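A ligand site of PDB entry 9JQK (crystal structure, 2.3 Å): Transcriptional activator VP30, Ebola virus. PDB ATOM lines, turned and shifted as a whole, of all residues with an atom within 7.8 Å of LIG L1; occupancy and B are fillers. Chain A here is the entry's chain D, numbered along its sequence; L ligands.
Trp 120 touches LIG L1 (CD1 to O2, 3.3 Å).
Hydrophobic or aromatic side chains within 4 Å of LIG L1: Trp 120.
The nearest printed residue that does not touch LIG L1 is Gln 119 (4.3 Å).
O3 of LIG L1 lies within hydrogen-bond range of OG of Ser 124 (2.7 Å).
OD1 of Asp 121 lies close to O1 of LIG L1, at 2.9 Å.
An oxygen (O1) of LG2 L2 sits close to the side-chain amide oxygen (OE1) of Gln 119, 3.2 Å away.
The side-chain carboxylate (OD1) of Asp 121 is in hydrogen-bond range of the side-chain hydroxyl (OG) of Ser 124, at 3.2 Å.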
ATOM      1  N   LEU A  89      -7.301  30.844 -11.933  1.00  0.00           N
ATOM      2  CA  LEU A  89      -8.039  29.644 -11.539  1.00  0.00           C
ATOM      3  C   LEU A  89      -8.934  29.997 -10.353  1.00  0.00           C
ATOM      4  O   LEU A  89      -8.631  30.900  -9.582  1.00  0.00           O
ATOM      5  CB  LEU A  89      -7.071  28.530 -11.172  1.00  0.00           C
ATOM      6  CG  LEU A  89      -6.051  28.130 -12.246  1.00  0.00           C
ATOM      7  CD1 LEU A  89      -5.094  27.083 -11.710  1.00  0.00           C
ATOM      8  CD2 LEU A  89      -6.734  27.620 -13.512  1.00  0.00           C
ATOM      9  N   GLN A  93      -9.712  25.155  -7.069  1.00  0.00           N
ATOM     10  CA  GLN A  93      -8.478  24.509  -7.519  1.00  0.00           C
ATOM     11  C   GLN A  93      -7.371  24.686  -6.471  1.00  0.00           C
ATOM     12  O   GLN A  93      -6.229  24.325  -6.732  1.00  0.00           O
ATOM     13  CB  GLN A  93      -8.047  25.065  -8.874  1.00  0.00           C
ATOM     14  CG  GLN A  93      -9.090  24.897  -9.970  1.00  0.00           C
ATOM     15  CD  GLN A  93      -9.557  23.471 -10.113  1.00  0.00           C
ATOM     16  OE1 GLN A  93     -10.725  23.154  -9.883  1.00  0.00           O
ATOM     17  NE2 GLN A  93      -8.627  22.580 -10.439  1.00  0.00           N
ATOM     18  N   PRO A  96      -6.229  20.906  -5.145  1.00  0.00           N
ATOM     19  CA  PRO A  96      -5.418  20.128  -6.103  1.00  0.00           C
ATOM     20  C   PRO A  96      -4.074  20.746  -6.484  1.00  0.00           C
ATOM     21  O   PRO A  96      -3.098  20.036  -6.680  1.00  0.00           O
ATOM     22  CB  PRO A  96      -6.362  19.978  -7.325  1.00  0.00           C
ATOM     23  CG  PRO A  96      -7.320  21.138  -7.205  1.00  0.00           C
ATOM     24  CD  PRO A  96      -7.521  21.319  -5.718  1.00  0.00           C
ATOM     25  N   VAL A  97      -4.032  22.090  -6.599  1.00  0.00           N
ATOM     26  CA  VAL A  97      -2.797  22.783  -6.951  1.00  0.00           C
ATOM     27  C   VAL A  97      -1.803  22.671  -5.787  1.00  0.00           C
ATOM     28  O   VAL A  97      -0.609  22.433  -6.003  1.00  0.00           O
ATOM     29  CB  VAL A  97      -3.050  24.259  -7.345  1.00  0.00           C
ATOM     30  CG1 VAL A  97      -1.753  25.063  -7.415  1.00  0.00           C
ATOM     31  CG2 VAL A  97      -3.804  24.365  -8.661  1.00  0.00           C
ATOM     32  N   VAL A 100      -0.228  19.223  -5.616  1.00  0.00           N
ATOM     33  CA  VAL A 100       0.808  19.045  -6.618  1.00  0.00           C
ATOM     34  C   VAL A 100       2.134  19.558  -6.058  1.00  0.00           C
ATOM     35  O   VAL A 100       3.165  18.924  -6.226  1.00  0.00           O
ATOM     36  CB  VAL A 100       0.459  19.724  -7.959  1.00  0.00           C
ATOM     37  CG1 VAL A 100       1.667  19.782  -8.903  1.00  0.00           C
ATOM     38  CG2 VAL A 100      -0.717  19.050  -8.655  1.00  0.00           C
ATOM     39  N   LEU A 116       2.868  12.523 -12.541  1.00  0.00           N
ATOM     40  CA  LEU A 116       2.311  13.777 -13.014  1.00  0.00           C
ATOM     41  C   LEU A 116       2.517  13.890 -14.531  1.00  0.00           C
ATOM     42  O   LEU A 116       1.619  14.314 -15.244  1.00  0.00           O
ATOM     43  CB  LEU A 116       2.971  14.943 -12.259  1.00  0.00           C
ATOM     44  CG  LEU A 116       2.395  16.339 -12.523  1.00  0.00           C
ATOM     45  CD1 LEU A 116       0.943  16.447 -12.045  1.00  0.00           C
ATOM     46  CD2 LEU A 116       3.259  17.400 -11.867  1.00  0.00           C
ATOM     47  N   GLN A 119       0.080  11.243 -16.309  1.00  0.00           N
ATOM     48  CA  GLN A 119      -1.355  11.423 -16.138  1.00  0.00           C
ATOM     49  C   GLN A 119      -1.845  12.662 -16.878  1.00  0.00           C
ATOM     50  O   GLN A 119      -2.957  12.673 -17.414  1.00  0.00           O
ATOM     51  CB  GLN A 119      -1.692  11.480 -14.641  1.00  0.00           C
ATOM     52  CG  GLN A 119      -3.181  11.620 -14.347  1.00  0.00           C
ATOM     53  CD  GLN A 119      -3.478  11.623 -12.870  1.00  0.00           C
ATOM     54  OE1 GLN A 119      -3.099  10.700 -12.139  1.00  0.00           O
ATOM     55  NE2 GLN A 119      -4.129  12.674 -12.409  1.00  0.00           N
ATOM     56  N   TRP A 120      -1.038  13.726 -16.881  1.00  0.00           N
ATOM     57  CA  TRP A 120      -1.449  15.001 -17.464  1.00  0.00           C
ATOM     58  C   TRP A 120      -1.093  15.058 -18.946  1.00  0.00           C
ATOM     59  O   TRP A 120      -0.126  14.459 -19.392  1.00  0.00           O
ATOM     60  CB  TRP A 120      -0.808  16.176 -16.704  1.00  0.00           C
ATOM     61  CG  TRP A 120      -1.469  16.478 -15.380  1.00  0.00           C
ATOM     62  CD1 TRP A 120      -2.309  15.670 -14.668  1.00  0.00           C
ATOM     63  CD2 TRP A 120      -1.276  17.657 -14.577  1.00  0.00           C
ATOM     64  NE1 TRP A 120      -2.690  16.290 -13.507  1.00  0.00           N
ATOM     65  CE2 TRP A 120      -2.065  17.504 -13.416  1.00  0.00           C
ATOM     66  CE3 TRP A 120      -0.516  18.838 -14.732  1.00  0.00           C
ATOM     67  CZ2 TRP A 120      -2.107  18.469 -12.418  1.00  0.00           C
ATOM     68  CZ3 TRP A 120      -0.563  19.795 -13.733  1.00  0.00           C
ATOM     69  CH2 TRP A 120      -1.351  19.605 -12.597  1.00  0.00           C
ATOM     70  N   ASP A 121      -1.915  15.809 -19.696  1.00  0.00           N
ATOM     71  CA  ASP A 121      -1.670  16.048 -21.106  1.00  0.00           C
ATOM     72  C   ASP A 121      -0.629  17.165 -21.241  1.00  0.00           C
ATOM     73  O   ASP A 121      -0.332  17.858 -20.272  1.00  0.00           O
ATOM     74  CB  ASP A 121      -2.961  16.354 -21.851  1.00  0.00           C
ATOM     75  CG  ASP A 121      -3.835  17.447 -21.241  1.00  0.00           C
ATOM     76  OD1 ASP A 121      -4.268  17.270 -20.083  1.00  0.00           O
ATOM     77  OD2 ASP A 121      -4.054  18.455 -21.918  1.00  0.00           O
ATOM     78  N   ARG A 122      -0.138  17.352 -22.469  1.00  0.00           N
ATOM     79  CA  ARG A 122       1.031  18.175 -22.733  1.00  0.00           C
ATOM     80  C   ARG A 122       0.740  19.644 -22.393  1.00  0.00           C
ATOM     81  O   ARG A 122       1.539  20.292 -21.732  1.00  0.00           O
ATOM     82  CB  ARG A 122       1.459  17.969 -24.186  1.00  0.00           C
ATOM     83  CG  ARG A 122       2.785  18.619 -24.543  1.00  0.00           C
ATOM     84  CD  ARG A 122       3.353  18.085 -25.856  1.00  0.00           C
ATOM     85  NE  ARG A 122       4.561  18.809 -26.256  1.00  0.00           N
ATOM     86  CZ  ARG A 122       4.592  20.084 -26.655  1.00  0.00           C
ATOM     87  NH1 ARG A 122       3.476  20.768 -26.811  1.00  0.00           N
ATOM     88  NH2 ARG A 122       5.756  20.651 -26.945  1.00  0.00           N
ATOM     89  N   GLN A 123      -0.419  20.150 -22.850  1.00  0.00           N
ATOM     90  CA  GLN A 123      -0.760  21.558 -22.684  1.00  0.00           C
ATOM     91  C   GLN A 123      -0.875  21.910 -21.192  1.00  0.00           C
ATOM     92  O   GLN A 123      -0.442  22.982 -20.778  1.00  0.00           O
ATOM     93  CB  GLN A 123      -2.036  21.944 -23.445  1.00  0.00           C
ATOM     94  CG  GLN A 123      -3.250  21.069 -23.134  1.00  0.00           C
ATOM     95  CD  GLN A 123      -4.550  21.648 -23.642  1.00  0.00           C
ATOM     96  OE1 GLN A 123      -4.694  21.993 -24.818  1.00  0.00           O
ATOM     97  NE2 GLN A 123      -5.520  21.774 -22.745  1.00  0.00           N
ATOM     98  N   SER A 124      -1.451  20.997 -20.406  1.00  0.00           N
ATOM     99  CA  SER A 124      -1.675  21.249 -18.985  1.00  0.00           C
ATOM    100  C   SER A 124      -0.343  21.387 -18.258  1.00  0.00           C
ATOM    101  O   SER A 124      -0.215  22.208 -17.355  1.00  0.00           O
ATOM    102  CB  SER A 124      -2.515  20.164 -18.374  1.00  0.00           C
ATOM    103  OG  SER A 124      -3.857  20.233 -18.842  1.00  0.00           O
ATOM    104  N   LEU A 125       0.640  20.565 -18.647  1.00  0.00           N
ATOM    105  CA  LEU A 125       1.971  20.603 -18.050  1.00  0.00           C
ATOM    106  C   LEU A 125       2.667  21.900 -18.436  1.00  0.00           C
ATOM    107  O   LEU A 125       3.369  22.488 -17.622  1.00  0.00           O
ATOM    108  CB  LEU A 125       2.761  19.368 -18.474  1.00  0.00           C
ATOM    109  CG  LEU A 125       2.319  18.041 -17.866  1.00  0.00           C
ATOM    110  CD1 LEU A 125       2.890  16.852 -18.627  1.00  0.00           C
ATOM    111  CD2 LEU A 125       2.729  17.967 -16.397  1.00  0.00           C
ATOM    112  N   MET A 127       1.341  24.896 -19.174  1.00  0.00           N
ATOM    113  CA  MET A 127       0.780  26.032 -18.449  1.00  0.00           C
ATOM    114  C   MET A 127       1.218  26.001 -16.978  1.00  0.00           C
ATOM    115  O   MET A 127       1.491  27.054 -16.390  1.00  0.00           O
ATOM    116  CB  MET A 127      -0.750  26.061 -18.557  1.00  0.00           C
ATOM    117  CG  MET A 127      -1.254  26.921 -19.713  1.00  0.00           C
ATOM    118  SD  MET A 127      -2.974  26.583 -20.147  1.00  0.00           S
ATOM    119  CE  MET A 127      -2.737  25.183 -21.247  1.00  0.00           C
HETATM  120  C1  LIG L   1      -7.079  18.531 -13.097  1.00  0.00           C
HETATM  121  C2  LIG L   1      -7.034  17.176 -12.806  1.00  0.00           C
HETATM  122  C3  LIG L   1      -6.480  16.292 -13.705  1.00  0.00           C
HETATM  123  C4  LIG L   1      -5.941  16.758 -14.909  1.00  0.00           C
HETATM  124  C5  LIG L   1      -6.635  20.551 -14.512  1.00  0.00           C
HETATM  125  C6  LIG L   1      -8.940  20.571 -15.638  1.00  0.00           C
HETATM  126  C7  LIG L   1      -9.158  21.206 -19.171  1.00  0.00           C
HETATM  127  C8  LIG L   1     -10.861  19.367 -19.683  1.00  0.00           C
HETATM  128  C9  LIG L   1     -13.168  20.144 -19.076  1.00  0.00           C
HETATM  129  C10 LIG L   1     -14.096  21.650 -21.915  1.00  0.00           C
HETATM  130  C11 LIG L   1     -13.143  20.928 -22.867  1.00  0.00           C
HETATM  131  C12 LIG L   1     -13.805  19.883 -23.744  1.00  0.00           C
HETATM  132  C13 LIG L   1     -12.151  19.708 -25.667  1.00  0.00           C
HETATM  133  O1  LIG L   1      -4.738  17.796 -17.231  1.00  0.00           O
HETATM  134  C14 LIG L   1      -5.382  18.622 -16.549  1.00  0.00           C
HETATM  135  C15 LIG L   1      -5.967  18.136 -15.210  1.00  0.00           C
HETATM  136  C16 LIG L   1      -6.571  19.035 -14.293  1.00  0.00           C
HETATM  137  O2  LIG L   1      -5.396  15.850 -15.756  1.00  0.00           O
HETATM  138  C17 LIG L   1      -8.049  21.112 -14.517  1.00  0.00           C
HETATM  139  C18 LIG L   1      -9.359  21.616 -16.656  1.00  0.00           C
HETATM  140  C19 LIG L   1      -8.473  21.672 -17.893  1.00  0.00           C
HETATM  141  C20 LIG L   1      -9.451  19.721 -19.207  1.00  0.00           C
HETATM  142  C21 LIG L   1     -11.919  19.463 -18.608  1.00  0.00           C
HETATM  143  C22 LIG L   1     -13.814  19.857 -20.168  1.00  0.00           C
HETATM  144  C23 LIG L   1     -14.762  20.748 -20.884  1.00  0.00           C
HETATM  145  C24 LIG L   1     -12.833  19.005 -24.504  1.00  0.00           C
HETATM  146  O3  LIG L   1      -5.613  19.781 -16.903  1.00  0.00           O
HETATM  147  C1  LG2 L   2      -1.389  14.296  -9.086  1.00  0.00           C
HETATM  148  C2  LG2 L   2      -1.741  15.584  -8.734  1.00  0.00           C
HETATM  149  C3  LG2 L   2      -3.031  15.880  -8.386  1.00  0.00           C
HETATM  150  C4  LG2 L   2      -4.003  14.882  -8.391  1.00  0.00           C
HETATM  151  C5  LG2 L   2      -1.852  11.866  -9.475  1.00  0.00           C
HETATM  152  C6  LG2 L   2      -2.094   9.795  -7.974  1.00  0.00           C
HETATM  153  C7  LG2 L   2      -0.101   7.498  -9.575  1.00  0.00           C
HETATM  154  C8  LG2 L   2       1.545   6.714  -7.778  1.00  0.00           C
HETATM  155  C9  LG2 L   2       0.270   4.575  -8.175  1.00  0.00           C
HETATM  156  C10 LG2 L   2       1.901   2.540  -9.954  1.00  0.00           C
HETATM  157  C11 LG2 L   2       1.035   2.922 -11.160  1.00  0.00           C
HETATM  158  C12 LG2 L   2       1.792   3.593 -12.286  1.00  0.00           C
HETATM  159  C13 LG2 L   2       2.567   3.272 -14.672  1.00  0.00           C
HETATM  160  O1  LG2 L   2      -4.566  11.487  -9.457  1.00  0.00           O
HETATM  161  C14 LG2 L   2      -4.755  12.490  -8.763  1.00  0.00           C
HETATM  162  C15 LG2 L   2      -3.667  13.558  -8.740  1.00  0.00           C
HETATM  163  C16 LG2 L   2      -2.331  13.270  -9.122  1.00  0.00           C
HETATM  164  O2  LG2 L   2      -5.285  15.238  -8.072  1.00  0.00           O
HETATM  165  C17 LG2 L   2      -1.327  11.079  -8.277  1.00  0.00           C
HETATM  166  C18 LG2 L   2      -2.246   8.823  -9.158  1.00  0.00           C
HETATM  167  C19 LG2 L   2      -0.996   8.638 -10.006  1.00  0.00           C
HETATM  168  C20 LG2 L   2       0.331   7.568  -8.124  1.00  0.00           C
HETATM  169  C21 LG2 L   2       1.544   5.332  -8.384  1.00  0.00           C
HETATM  170  C22 LG2 L   2       0.079   3.281  -8.358  1.00  0.00           C
HETATM  171  C23 LG2 L   2       1.132   2.267  -8.685  1.00  0.00           C
HETATM  172  C24 LG2 L   2       2.371   2.650 -13.313  1.00  0.00           C
HETATM  173  O3  LG2 L   2      -5.761  12.669  -8.045  1.00  0.00           O
